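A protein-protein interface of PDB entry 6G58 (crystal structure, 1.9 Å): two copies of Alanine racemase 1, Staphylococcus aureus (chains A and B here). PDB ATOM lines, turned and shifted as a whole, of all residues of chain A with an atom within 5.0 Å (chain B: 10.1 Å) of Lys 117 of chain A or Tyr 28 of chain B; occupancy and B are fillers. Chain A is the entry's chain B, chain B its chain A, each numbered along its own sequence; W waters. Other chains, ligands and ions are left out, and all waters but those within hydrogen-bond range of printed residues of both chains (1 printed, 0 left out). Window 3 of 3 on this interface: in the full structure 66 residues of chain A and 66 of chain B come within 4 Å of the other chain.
N of Tyr 28 of chain B sits at hydrogen-bond distance from OD2 of Asp 90 of chain A, 2.9 Å away.
ND2 of Asn 400 of chain B sits at hydrogen-bond distance from OD2 of Asp 90 of chain A (2.9 Å).
Among the printed residues, pairs that only touch across the chains: Leu 89 of chain A with Tyr 28 of chain B, Asp 90 of chain A with Tyr 27 of chain B, Asp 90 of chain A with Arg 29 of chain B, Asp 90 of chain A with Leu 402 of chain B, Asp 90 of chain A with Leu 403 of chain B, Ile 93 of chain A with Tyr 28 of chain B, Ile 93 of chain A with Leu 403 of chain B, Leu 110 of chain A with Tyr 28 of chain B, Pro 111 of chain A with Tyr 28 of chain B, Asp 114 of chain A with Tyr 28 of chain B and Lys 117 of chain A with Tyr 28 of chain B.
Water W1 lies within hydrogen-bond range of O of Tyr 28 of chain B (2.7 Å) and N of Leu 89 of chain A (2.9 Å).
The side-chain carboxylate (OD2) of Asp 25 of chain B is in hydrogen-bond range of the backbone NH (N) of Asn 400 of chain B, at 2.7 Å.
The side-chain amide nitrogen of Asn 400 of chain B is in hydrogen-bond range of the backbone carbonyl oxygen of Lys 26 of chain B (2.9 Å).
NH1 of Arg 29 of chain B sits at hydrogen-bond distance from O of Pro 303 of chain B (3.2 Å).
OD1 of Asn 400 of chain B sits close to N of Leu 402 of chain B.
The side-chain amino group of Lys 117 of chain A lies within hydrogen-bond range of the side-chain amide oxygen of Gln 120 of chain A.
Printed residues of chain A that touch a printed residue of chain B: Leu 89, Asp 90, Ile 93, Leu 110, Pro 111, Asp 114 and Lys 117.
Hydrophobic or aromatic side chains of chain A within 4 Å of the printed part of chain B: Leu 89, Ile 93, Leu 110 and Pro 111.
Of the 23 printed residues of chain B, 6 touch a printed residue of chain A.
Printed residues of chain B that touch a printed residue of chain A: Tyr 27, Tyr 28, Arg 29, Asn 400, Leu 402 and Leu 403.
Printed residues of chain B within 4 Å of Asp 90 of chain A: Tyr 27 (3.3 Å), Tyr 28 (2.9 Å), Arg 29 (3.6 Å), Asn 400 (2.9 Å), Leu 402 (3.8 Å) and Leu 403 (3.7 Å).
Printed residues of chain B within 4 Å of Ile 93 of chain A: Tyr 28 (3.7 Å) and Leu 403 (3.8 Å).
No residue of chain B comes within 4 Å of Asp 116 of chain A.
No residue of chain B comes within 4 Å of Ala 118 of chain A.
Ile 119 of chain A touches none of the printed residues of chain B.
No residue of chain B comes within 4 Å of Gln 120 of chain A.
No residue of chain B comes within 4 Å of His 121 of chain A.
Tyr 28 of chain B touches just these residues of chain A: Leu 89 (3.9 Å), Asp 90 (2.9 Å), Ile 93 (3.7 Å), Leu 110 (3.8 Å), Pro 111 (3.5 Å), Asp 114 (3.6 Å) and Lys 117 (3.6 Å).
Val 398 of chain B touches none of the printed residues of chain A.
Printed residues of chain A within 4 Å of Leu 403 of chain B: Asp 90 and Ile 93.
No position is printed for both chains.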
ATOM      1  N   LEU A  89      -6.598  -4.971 -25.639  1.00  0.00           N
ATOM      2  CA  LEU A  89      -7.195  -3.710 -26.062  1.00  0.00           C
ATOM      3  C   LEU A  89      -7.284  -2.698 -24.901  1.00  0.00           C
ATOM      4  O   LEU A  89      -7.146  -1.514 -25.123  1.00  0.00           O
ATOM      5  CB  LEU A  89      -8.560  -3.919 -26.741  1.00  0.00           C
ATOM      6  CG  LEU A  89      -9.233  -2.636 -27.282  1.00  0.00           C
ATOM      7  CD1 LEU A  89      -8.347  -1.999 -28.318  1.00  0.00           C
ATOM      8  CD2 LEU A  89     -10.607  -2.916 -27.849  1.00  0.00           C
ATOM      9  N   ASP A  90      -7.509  -3.161 -23.675  1.00  0.00           N
ATOM     10  CA  ASP A  90      -7.512  -2.256 -22.510  1.00  0.00           C
ATOM     11  C   ASP A  90      -6.187  -1.492 -22.433  1.00  0.00           C
ATOM     12  O   ASP A  90      -6.165  -0.283 -22.209  1.00  0.00           O
ATOM     13  CB  ASP A  90      -7.774  -3.000 -21.179  1.00  0.00           C
ATOM     14  CG  ASP A  90      -8.942  -3.993 -21.275  1.00  0.00           C
ATOM     15  OD1 ASP A  90      -8.742  -5.157 -21.745  1.00  0.00           O
ATOM     16  OD2 ASP A  90     -10.055  -3.598 -20.898  1.00  0.00           O
ATOM     17  N   ILE A  93      -6.084   1.106 -25.282  1.00  0.00           N
ATOM     18  CA  ILE A  93      -6.951   2.237 -24.994  1.00  0.00           C
ATOM     19  C   ILE A  93      -6.319   3.101 -23.891  1.00  0.00           C
ATOM     20  O   ILE A  93      -6.356   4.336 -23.958  1.00  0.00           O
ATOM     21  CB  ILE A  93      -8.386   1.811 -24.626  1.00  0.00           C
ATOM     22  CG1 ILE A  93      -9.058   1.192 -25.869  1.00  0.00           C
ATOM     23  CG2 ILE A  93      -9.220   3.019 -24.138  1.00  0.00           C
ATOM     24  CD1 ILE A  93     -10.357   0.469 -25.587  1.00  0.00           C
ATOM     25  N   LEU A 110      -8.733 -10.277 -29.592  1.00  0.00           N
ATOM     26  CA  LEU A 110      -9.835  -9.450 -29.143  1.00  0.00           C
ATOM     27  C   LEU A 110     -11.143 -10.208 -29.286  1.00  0.00           C
ATOM     28  O   LEU A 110     -11.394 -10.806 -30.308  1.00  0.00           O
ATOM     29  CB  LEU A 110      -9.900  -8.168 -29.969  1.00  0.00           C
ATOM     30  CG  LEU A 110     -10.944  -7.166 -29.493  1.00  0.00           C
ATOM     31  CD1 LEU A 110     -10.534  -6.477 -28.211  1.00  0.00           C
ATOM     32  CD2 LEU A 110     -11.259  -6.157 -30.569  1.00  0.00           C
ATOM     33  N   PRO A 111     -11.999 -10.202 -28.247  1.00  0.00           N
ATOM     34  CA  PRO A 111     -13.365 -10.716 -28.514  1.00  0.00           C
ATOM     35  C   PRO A 111     -14.039 -10.003 -29.707  1.00  0.00           C
ATOM     36  O   PRO A 111     -14.017  -8.763 -29.789  1.00  0.00           O
ATOM     37  CB  PRO A 111     -14.109 -10.417 -27.214  1.00  0.00           C
ATOM     38  CG  PRO A 111     -13.037 -10.327 -26.170  1.00  0.00           C
ATOM     39  CD  PRO A 111     -11.838  -9.748 -26.856  1.00  0.00           C
ATOM     40  N   ASP A 114     -16.209  -6.796 -29.634  1.00  0.00           N
ATOM     41  CA  ASP A 114     -15.569  -5.510 -29.296  1.00  0.00           C
ATOM     42  C   ASP A 114     -14.838  -4.855 -30.468  1.00  0.00           C
ATOM     43  O   ASP A 114     -14.140  -3.858 -30.300  1.00  0.00           O
ATOM     44  CB  ASP A 114     -14.560  -5.729 -28.163  1.00  0.00           C
ATOM     45  CG  ASP A 114     -15.217  -6.134 -26.861  1.00  0.00           C
ATOM     46  OD1 ASP A 114     -16.336  -5.710 -26.578  1.00  0.00           O
ATOM     47  OD2 ASP A 114     -14.577  -6.886 -26.101  1.00  0.00           O
ATOM     48  N   ILE A 115     -15.011  -5.403 -31.662  1.00  0.00           N
ATOM     49  CA  ILE A 115     -14.268  -4.944 -32.850  1.00  0.00           C
ATOM     50  C   ILE A 115     -14.407  -3.452 -33.135  1.00  0.00           C
ATOM     51  O   ILE A 115     -13.438  -2.821 -33.470  1.00  0.00           O
ATOM     52  CB  ILE A 115     -14.664  -5.808 -34.100  1.00  0.00           C
ATOM     53  CG1 ILE A 115     -13.741  -5.563 -35.267  1.00  0.00           C
ATOM     54  CG2 ILE A 115     -16.088  -5.574 -34.557  1.00  0.00           C
ATOM     55  CD1 ILE A 115     -12.366  -6.143 -35.014  1.00  0.00           C
ATOM     56  N   ASP A 116     -15.606  -2.893 -32.977  1.00  0.00           N
ATOM     57  CA  ASP A 116     -15.835  -1.459 -33.249  1.00  0.00           C
ATOM     58  C   ASP A 116     -14.945  -0.545 -32.361  1.00  0.00           C
ATOM     59  O   ASP A 116     -14.570   0.533 -32.808  1.00  0.00           O
ATOM     60  CB  ASP A 116     -17.309  -1.064 -33.048  1.00  0.00           C
ATOM     61  CG  ASP A 116     -18.225  -1.412 -34.266  1.00  0.00           C
ATOM     62  OD1 ASP A 116     -17.758  -1.779 -35.364  1.00  0.00           O
ATOM     63  OD2 ASP A 116     -19.459  -1.280 -34.123  1.00  0.00           O
ATOM     64  N   LYS A 117     -14.629  -0.972 -31.125  1.00  0.00           N
ATOM     65  CA  LYS A 117     -13.775  -0.181 -30.233  1.00  0.00           C
ATOM     66  C   LYS A 117     -12.345  -0.121 -30.721  1.00  0.00           C
ATOM     67  O   LYS A 117     -11.715   0.926 -30.626  1.00  0.00           O
ATOM     68  CB  LYS A 117     -13.807  -0.693 -28.781  1.00  0.00           C
ATOM     69  CG  LYS A 117     -15.036  -0.256 -28.049  1.00  0.00           C
ATOM     70  CD  LYS A 117     -14.966   1.227 -27.647  1.00  0.00           C
ATOM     71  CE  LYS A 117     -16.349   1.746 -27.274  1.00  0.00           C
ATOM     72  NZ  LYS A 117     -16.382   3.217 -27.128  1.00  0.00           N
ATOM     73  N   ALA A 118     -11.847  -1.209 -31.277  1.00  0.00           N
ATOM     74  CA  ALA A 118     -10.519  -1.204 -31.875  1.00  0.00           C
ATOM     75  C   ALA A 118     -10.477  -0.259 -33.073  1.00  0.00           C
ATOM     76  O   ALA A 118      -9.529   0.532 -33.231  1.00  0.00           O
ATOM     77  CB  ALA A 118     -10.114  -2.593 -32.305  1.00  0.00           C
ATOM     78  N   ILE A 119     -11.519  -0.302 -33.888  1.00  0.00           N
ATOM     79  CA  ILE A 119     -11.607   0.587 -35.059  1.00  0.00           C
ATOM     80  C   ILE A 119     -11.645   2.023 -34.591  1.00  0.00           C
ATOM     81  O   ILE A 119     -10.906   2.869 -35.106  1.00  0.00           O
ATOM     82  CB  ILE A 119     -12.829   0.280 -35.964  1.00  0.00           C
ATOM     83  CG1 ILE A 119     -12.693  -1.128 -36.563  1.00  0.00           C
ATOM     84  CG2 ILE A 119     -12.948   1.321 -37.078  1.00  0.00           C
ATOM     85  CD1 ILE A 119     -13.941  -1.601 -37.291  1.00  0.00           C
ATOM     86  N   GLN A 120     -12.519   2.318 -33.630  1.00  0.00           N
ATOM     87  CA  GLN A 120     -12.675   3.672 -33.138  1.00  0.00           C
ATOM     88  C   GLN A 120     -11.366   4.254 -32.638  1.00  0.00           C
ATOM     89  O   GLN A 120     -11.070   5.400 -32.882  1.00  0.00           O
ATOM     90  CB  GLN A 120     -13.709   3.697 -31.993  1.00  0.00           C
ATOM     91  CG  GLN A 120     -13.982   5.064 -31.394  1.00  0.00           C
ATOM     92  CD  GLN A 120     -14.876   5.015 -30.144  1.00  0.00           C
ATOM     93  OE1 GLN A 120     -15.378   3.973 -29.719  1.00  0.00           O
ATOM     94  NE2 GLN A 120     -15.041   6.146 -29.547  1.00  0.00           N
ATOM     95  N   HIS A 121     -10.607   3.459 -31.888  1.00  0.00           N
ATOM     96  CA  HIS A 121      -9.351   3.920 -31.274  1.00  0.00           C
ATOM     97  C   HIS A 121      -8.110   3.724 -32.160  1.00  0.00           C
ATOM     98  O   HIS A 121      -6.998   3.980 -31.703  1.00  0.00           O
ATOM     99  CB  HIS A 121      -9.164   3.253 -29.898  1.00  0.00           C
ATOM    100  CG  HIS A 121     -10.121   3.751 -28.864  1.00  0.00           C
ATOM    101  ND1 HIS A 121      -9.985   4.980 -28.252  1.00  0.00           N
ATOM    102  CD2 HIS A 121     -11.226   3.178 -28.315  1.00  0.00           C
ATOM    103  CE1 HIS A 121     -10.978   5.151 -27.390  1.00  0.00           C
ATOM    104  NE2 HIS A 121     -11.754   4.079 -27.423  1.00  0.00           N
ATOM    105  N   SER B  24     -19.717   2.280 -13.918  1.00  0.00           N
ATOM    106  CA  SER B  24     -19.097   0.997 -14.346  1.00  0.00           C
ATOM    107  C   SER B  24     -18.157   1.072 -15.615  1.00  0.00           C
ATOM    108  O   SER B  24     -18.507   1.662 -16.656  1.00  0.00           O
ATOM    109  CB  SER B  24     -20.208  -0.064 -14.539  1.00  0.00           C
ATOM    110  OG  SER B  24     -19.712  -1.357 -14.327  1.00  0.00           O
ATOM    111  N   ASP B  25     -16.948   0.531 -15.454  1.00  0.00           N
ATOM    112  CA  ASP B  25     -15.945   0.496 -16.498  1.00  0.00           C
ATOM    113  C   ASP B  25     -16.298  -0.626 -17.495  1.00  0.00           C
ATOM    114  O   ASP B  25     -17.079  -1.538 -17.236  1.00  0.00           O
ATOM    115  CB  ASP B  25     -14.557   0.204 -15.945  1.00  0.00           C
ATOM    116  CG  ASP B  25     -13.978   1.310 -15.103  1.00  0.00           C
ATOM    117  OD1 ASP B  25     -14.133   2.506 -15.417  1.00  0.00           O
ATOM    118  OD2 ASP B  25     -13.293   0.955 -14.121  1.00  0.00           O
ATOM    119  N   LYS B  26     -15.728  -0.499 -18.668  1.00  0.00           N
ATOM    120  CA  LYS B  26     -15.738  -1.518 -19.686  1.00  0.00           C
ATOM    121  C   LYS B  26     -14.477  -2.346 -19.511  1.00  0.00           C
ATOM    122  O   LYS B  26     -13.581  -1.921 -18.794  1.00  0.00           O
ATOM    123  CB  LYS B  26     -15.759  -0.836 -21.036  1.00  0.00           C
ATOM    124  CG  LYS B  26     -17.051  -0.060 -21.340  1.00  0.00           C
ATOM    125  CD  LYS B  26     -18.270  -1.002 -21.304  1.00  0.00           C
ATOM    126  CE  LYS B  26     -19.515  -0.454 -21.997  1.00  0.00           C
ATOM    127  NZ  LYS B  26     -20.603  -1.477 -22.023  1.00  0.00           N
ATOM    128  N   TYR B  27     -14.443  -3.528 -20.100  1.00  0.00           N
ATOM    129  CA  TYR B  27     -13.224  -4.321 -20.174  1.00  0.00           C
ATOM    130  C   TYR B  27     -13.256  -5.127 -21.482  1.00  0.00           C
ATOM    131  O   TYR B  27     -14.315  -5.481 -21.970  1.00  0.00           O
ATOM    132  CB  TYR B  27     -13.041  -5.165 -18.925  1.00  0.00           C
ATOM    133  CG  TYR B  27     -14.006  -6.270 -18.786  1.00  0.00           C
ATOM    134  CD1 TYR B  27     -15.328  -6.040 -18.364  1.00  0.00           C
ATOM    135  CD2 TYR B  27     -13.619  -7.571 -19.045  1.00  0.00           C
ATOM    136  CE1 TYR B  27     -16.233  -7.092 -18.251  1.00  0.00           C
ATOM    137  CE2 TYR B  27     -14.519  -8.617 -18.924  1.00  0.00           C
ATOM    138  CZ  TYR B  27     -15.817  -8.368 -18.531  1.00  0.00           C
ATOM    139  OH  TYR B  27     -16.652  -9.443 -18.433  1.00  0.00           O
ATOM    140  N   TYR B  28     -12.081  -5.381 -22.025  1.00  0.00           N
ATOM    141  CA  TYR B  28     -11.936  -5.835 -23.387  1.00  0.00           C
ATOM    142  C   TYR B  28     -11.118  -7.144 -23.509  1.00  0.00           C
ATOM    143  O   TYR B  28     -10.564  -7.445 -24.574  1.00  0.00           O
ATOM    144  CB  TYR B  28     -11.332  -4.697 -24.184  1.00  0.00           C
ATOM    145  CG  TYR B  28     -12.270  -3.514 -24.259  1.00  0.00           C
ATOM    146  CD1 TYR B  28     -13.431  -3.571 -25.019  1.00  0.00           C
ATOM    147  CD2 TYR B  28     -12.026  -2.346 -23.524  1.00  0.00           C
ATOM    148  CE1 TYR B  28     -14.322  -2.491 -25.069  1.00  0.00           C
ATOM    149  CE2 TYR B  28     -12.904  -1.268 -23.558  1.00  0.00           C
ATOM    150  CZ  TYR B  28     -14.062  -1.349 -24.304  1.00  0.00           C
ATOM    151  OH  TYR B  28     -14.922  -0.281 -24.365  1.00  0.00           O
ATOM    152  N   ARG B  29     -11.039  -7.893 -22.419  1.00  0.00           N
ATOM    153  CA  ARG B  29     -10.419  -9.211 -22.416  1.00  0.00           C
ATOM    154  C   ARG B  29     -11.208 -10.045 -21.450  1.00  0.00           C
ATOM    155  O   ARG B  29     -11.449  -9.582 -20.347  1.00  0.00           O
ATOM    156  CB  ARG B  29      -8.942  -9.145 -21.993  1.00  0.00           C
ATOM    157  CG  ARG B  29      -8.260 -10.522 -21.880  1.00  0.00           C
ATOM    158  CD  ARG B  29      -6.837 -10.442 -21.379  1.00  0.00           C
ATOM    159  NE  ARG B  29      -6.857  -9.997 -19.992  1.00  0.00           N
ATOM    160  CZ  ARG B  29      -5.889 -10.188 -19.094  1.00  0.00           C
ATOM    161  NH1 ARG B  29      -4.756 -10.806 -19.401  1.00  0.00           N
ATOM    162  NH2 ARG B  29      -6.082  -9.753 -17.866  1.00  0.00           N
ATOM    163  N   SER B  30     -11.549 -11.278 -21.819  1.00  0.00           N
ATOM    164  CA  SER B  30     -12.400 -12.107 -20.953  1.00  0.00           C
ATOM    165  C   SER B  30     -11.603 -12.872 -19.891  1.00  0.00           C
ATOM    166  O   SER B  30     -11.512 -14.097 -19.905  1.00  0.00           O
ATOM    167  CB  SER B  30     -13.322 -13.037 -21.755  1.00  0.00           C
ATOM    168  OG  SER B  30     -14.511 -13.293 -20.990  1.00  0.00           O
ATOM    169  N   ALA B  31     -11.044 -12.112 -18.957  1.00  0.00           N
ATOM    170  CA  ALA B  31     -10.365 -12.628 -17.778  1.00  0.00           C
ATOM    171  C   ALA B  31     -10.644 -11.607 -16.674  1.00  0.00           C
ATOM    172  O   ALA B  31     -10.461 -10.412 -16.872  1.00  0.00           O
ATOM    173  CB  ALA B  31      -8.856 -12.754 -17.999  1.00  0.00           C
ATOM    174  N   TYR B  32     -11.107 -12.075 -15.525  1.00  0.00           N
ATOM    175  CA  TYR B  32     -11.595 -11.173 -14.518  1.00  0.00           C
ATOM    176  C   TYR B  32     -11.753 -11.875 -13.200  1.00  0.00           C
ATOM    177  O   TYR B  32     -11.739 -13.102 -13.137  1.00  0.00           O
ATOM    178  CB  TYR B  32     -12.933 -10.518 -14.975  1.00  0.00           C
ATOM    179  CG  TYR B  32     -14.023 -11.500 -15.292  1.00  0.00           C
ATOM    180  CD1 TYR B  32     -14.896 -11.934 -14.306  1.00  0.00           C
ATOM    181  CD2 TYR B  32     -14.205 -11.979 -16.583  1.00  0.00           C
ATOM    182  CE1 TYR B  32     -15.892 -12.853 -14.599  1.00  0.00           C
ATOM    183  CE2 TYR B  32     -15.203 -12.901 -16.883  1.00  0.00           C
ATOM    184  CZ  TYR B  32     -16.045 -13.327 -15.882  1.00  0.00           C
ATOM    185  OH  TYR B  32     -17.053 -14.231 -16.129  1.00  0.00           O
ATOM    186  N   VAL B 274     -10.313 -18.732 -25.393  1.00  0.00           N
ATOM    187  CA  VAL B 274     -10.295 -17.923 -26.599  1.00  0.00           C
ATOM    188  C   VAL B 274     -10.571 -18.819 -27.792  1.00  0.00           C
ATOM    189  O   VAL B 274     -11.470 -18.545 -28.577  1.00  0.00           O
ATOM    190  CB  VAL B 274      -8.950 -17.176 -26.783  1.00  0.00           C
ATOM    191  CG1 VAL B 274      -8.852 -16.606 -28.162  1.00  0.00           C
ATOM    192  CG2 VAL B 274      -8.839 -16.057 -25.789  1.00  0.00           C
ATOM    193  N   PRO B 303      -6.803 -16.290 -21.908  1.00  0.00           N
ATOM    194  CA  PRO B 303      -6.228 -14.963 -21.954  1.00  0.00           C
ATOM    195  C   PRO B 303      -5.892 -14.460 -20.543  1.00  0.00           C
ATOM    196  O   PRO B 303      -6.403 -13.436 -20.096  1.00  0.00           O
ATOM    197  CB  PRO B 303      -7.344 -14.149 -22.625  1.00  0.00           C
ATOM    198  CG  PRO B 303      -8.587 -14.757 -22.046  1.00  0.00           C
ATOM    199  CD  PRO B 303      -8.284 -16.222 -21.950  1.00  0.00           C
ATOM    200  N   ARG B 385      -4.267  -5.539 -13.739  1.00  0.00           N
ATOM    201  CA  ARG B 385      -4.790  -5.772 -15.078  1.00  0.00           C
ATOM    202  C   ARG B 385      -6.114  -6.529 -15.058  1.00  0.00           C
ATOM    203  O   ARG B 385      -6.891  -6.431 -16.015  1.00  0.00           O
ATOM    204  CB  ARG B 385      -3.773  -6.498 -15.955  1.00  0.00           C
ATOM    205  CG  ARG B 385      -4.172  -6.472 -17.432  1.00  0.00           C
ATOM    206  CD  ARG B 385      -3.041  -6.845 -18.373  1.00  0.00           C
ATOM    207  NE  ARG B 385      -2.594  -8.230 -18.174  1.00  0.00           N
ATOM    208  CZ  ARG B 385      -1.634  -8.800 -18.876  1.00  0.00           C
ATOM    209  NH1 ARG B 385      -0.989  -8.123 -19.843  1.00  0.00           N
ATOM    210  NH2 ARG B 385      -1.292 -10.050 -18.612  1.00  0.00           N
ATOM    211  N   LEU B 386      -6.399  -7.265 -13.972  1.00  0.00           N
ATOM    212  CA  LEU B 386      -7.672  -7.949 -13.868  1.00  0.00           C
ATOM    213  C   LEU B 386      -8.798  -7.004 -13.478  1.00  0.00           C
ATOM    214  O   LEU B 386      -8.771  -6.410 -12.404  1.00  0.00           O
ATOM    215  CB  LEU B 386      -7.619  -9.103 -12.853  1.00  0.00           C
ATOM    216  CG  LEU B 386      -6.743 -10.263 -13.249  1.00  0.00           C
ATOM    217  CD1 LEU B 386      -6.481 -11.085 -11.989  1.00  0.00           C
ATOM    218  CD2 LEU B 386      -7.388 -11.103 -14.333  1.00  0.00           C
ATOM    219  N   PRO B 387      -9.827  -6.915 -14.319  1.00  0.00           N
ATOM    220  CA  PRO B 387     -11.024  -6.205 -13.818  1.00  0.00           C
ATOM    221  C   PRO B 387     -11.630  -6.913 -12.581  1.00  0.00           C
ATOM    222  O   PRO B 387     -11.566  -8.133 -12.488  1.00  0.00           O
ATOM    223  CB  PRO B 387     -12.003  -6.290 -15.001  1.00  0.00           C
ATOM    224  CG  PRO B 387     -11.127  -6.587 -16.191  1.00  0.00           C
ATOM    225  CD  PRO B 387     -10.026  -7.441 -15.678  1.00  0.00           C
ATOM    226  N   ILE B 389     -15.220  -7.489 -10.969  1.00  0.00           N
ATOM    227  CA  ILE B 389     -16.640  -7.411 -11.221  1.00  0.00           C
ATOM    228  C   ILE B 389     -17.371  -7.706  -9.908  1.00  0.00           C
ATOM    229  O   ILE B 389     -17.344  -8.841  -9.400  1.00  0.00           O
ATOM    230  CB  ILE B 389     -17.039  -8.400 -12.319  1.00  0.00           C
ATOM    231  CG1 ILE B 389     -16.144  -8.194 -13.567  1.00  0.00           C
ATOM    232  CG2 ILE B 389     -18.496  -8.207 -12.673  1.00  0.00           C
ATOM    233  CD1 ILE B 389     -16.658  -8.895 -14.823  1.00  0.00           C
ATOM    234  N   ARG B 396     -24.444  -5.543 -10.660  1.00  0.00           N
ATOM    235  CA  ARG B 396     -23.150  -5.894 -11.174  1.00  0.00           C
ATOM    236  C   ARG B 396     -22.451  -4.563 -11.468  1.00  0.00           C
ATOM    237  O   ARG B 396     -23.078  -3.652 -12.010  1.00  0.00           O
ATOM    238  CB  ARG B 396     -23.370  -6.738 -12.438  1.00  0.00           C
ATOM    239  CG  ARG B 396     -22.152  -6.973 -13.298  1.00  0.00           C
ATOM    240  CD  ARG B 396     -22.538  -7.529 -14.672  1.00  0.00           C
ATOM    241  NE  ARG B 396     -21.447  -7.526 -15.650  1.00  0.00           N
ATOM    242  CZ  ARG B 396     -21.000  -6.448 -16.311  1.00  0.00           C
ATOM    243  NH1 ARG B 396     -21.502  -5.224 -16.096  1.00  0.00           N
ATOM    244  NH2 ARG B 396     -20.036  -6.597 -17.224  1.00  0.00           N
ATOM    245  N   VAL B 398     -18.317  -2.915 -12.500  1.00  0.00           N
ATOM    246  CA  VAL B 398     -16.975  -3.266 -12.948  1.00  0.00           C
ATOM    247  C   VAL B 398     -15.968  -2.154 -12.660  1.00  0.00           C
ATOM    248  O   VAL B 398     -16.255  -1.009 -12.926  1.00  0.00           O
ATOM    249  CB  VAL B 398     -16.949  -3.521 -14.469  1.00  0.00           C
ATOM    250  CG1 VAL B 398     -15.547  -3.835 -14.948  1.00  0.00           C
ATOM    251  CG2 VAL B 398     -17.941  -4.626 -14.887  1.00  0.00           C
ATOM    252  N   THR B 399     -14.814  -2.506 -12.103  1.00  0.00           N
ATOM    253  CA  THR B 399     -13.658  -1.626 -11.990  1.00  0.00           C
ATOM    254  C   THR B 399     -12.546  -2.208 -12.858  1.00  0.00           C
ATOM    255  O   THR B 399     -12.190  -3.377 -12.729  1.00  0.00           O
ATOM    256  CB  THR B 399     -13.174  -1.513 -10.532  1.00  0.00           C
ATOM    257  OG1 THR B 399     -14.222  -0.921  -9.757  1.00  0.00           O
ATOM    258  CG2 THR B 399     -11.923  -0.598 -10.426  1.00  0.00           C
ATOM    259  N   ASN B 400     -12.001  -1.382 -13.743  1.00  0.00           N
ATOM    260  CA  ASN B 400     -10.906  -1.789 -14.614  1.00  0.00           C
ATOM    261  C   ASN B 400      -9.909  -0.659 -14.482  1.00  0.00           C
ATOM    262  O   ASN B 400     -10.116   0.419 -15.051  1.00  0.00           O
ATOM    263  CB  ASN B 400     -11.436  -1.959 -16.036  1.00  0.00           C
ATOM    264  CG  ASN B 400     -10.341  -2.282 -17.057  1.00  0.00           C
ATOM    265  OD1 ASN B 400      -9.159  -2.383 -16.714  1.00  0.00           O
ATOM    266  ND2 ASN B 400     -10.744  -2.484 -18.316  1.00  0.00           N
ATOM    267  N   GLU B 401      -8.849  -0.902 -13.727  1.00  0.00           N
ATOM    268  CA  GLU B 401      -7.849   0.115 -13.360  1.00  0.00           C
ATOM    269  C   GLU B 401      -7.177   0.756 -14.573  1.00  0.00           C
ATOM    270  O   GLU B 401      -6.829   1.923 -14.519  1.00  0.00           O
ATOM    271  CB  GLU B 401      -6.792  -0.573 -12.497  1.00  0.00           C
ATOM    272  CG  GLU B 401      -5.620   0.241 -11.990  1.00  0.00           C
ATOM    273  CD  GLU B 401      -5.964   1.026 -10.747  1.00  0.00           C
ATOM    274  OE1 GLU B 401      -6.135   0.365  -9.670  1.00  0.00           O
ATOM    275  OE2 GLU B 401      -6.014   2.287 -10.875  1.00  0.00           O
ATOM    276  N   LEU B 402      -7.016  -0.006 -15.661  1.00  0.00           N
ATOM    277  CA  LEU B 402      -6.359   0.485 -16.868  1.00  0.00           C
ATOM    278  C   LEU B 402      -7.119   1.628 -17.492  1.00  0.00           C
ATOM    279  O   LEU B 402      -6.520   2.470 -18.127  1.00  0.00           O
ATOM    280  CB  LEU B 402      -6.191  -0.638 -17.887  1.00  0.00           C
ATOM    281  CG  LEU B 402      -4.921  -1.494 -17.690  1.00  0.00           C
ATOM    282  CD1 LEU B 402      -4.868  -2.114 -16.312  1.00  0.00           C
ATOM    283  CD2 LEU B 402      -4.873  -2.550 -18.793  1.00  0.00           C
ATOM    284  N   LEU B 403      -8.448   1.648 -17.342  1.00  0.00           N
ATOM    285  CA  LEU B 403      -9.293   2.667 -17.959  1.00  0.00           C
ATOM    286  C   LEU B 403      -9.767   3.754 -17.001  1.00  0.00           C
ATOM    287  O   LEU B 403     -10.592   4.560 -17.384  1.00  0.00           O
ATOM    288  CB  LEU B 403     -10.483   1.990 -18.645  1.00  0.00           C
ATOM    289  CG  LEU B 403     -10.080   0.898 -19.650  1.00  0.00           C
ATOM    290  CD1 LEU B 403     -11.316   0.365 -20.354  1.00  0.00           C
ATOM    291  CD2 LEU B 403      -9.087   1.425 -20.686  1.00  0.00           C
ATOM    292  N   LYS B 404      -9.210   3.793 -15.791  1.00  0.00           N
ATOM    293  CA  LYS B 404      -9.626   4.685 -14.676  1.00  0.00           C
ATOM    294  C   LYS B 404      -8.830   5.949 -14.827  1.00  0.00           C
ATOM    295  O   LYS B 404      -9.357   7.055 -14.674  1.00  0.00           O
ATOM    296  CB  LYS B 404      -9.324   4.015 -13.311  1.00  0.00           C
ATOM    297  CG  LYS B 404      -9.385   4.872 -12.058  1.00  0.00           C
ATOM    298  CD  LYS B 404      -9.628   4.031 -10.778  1.00  0.00           C
ATOM    299  CE  LYS B 404      -9.328   4.811  -9.481  1.00  0.00           C
ATOM    300  NZ  LYS B 404     -10.194   6.019  -9.235  1.00  0.00           N
ATOM    301  OXT LYS B 404      -7.636   5.892 -15.106  1.00  0.00           O
HETATM  302  O   HOH W   1      -8.080  -7.484 -25.686  1.00  0.00           O
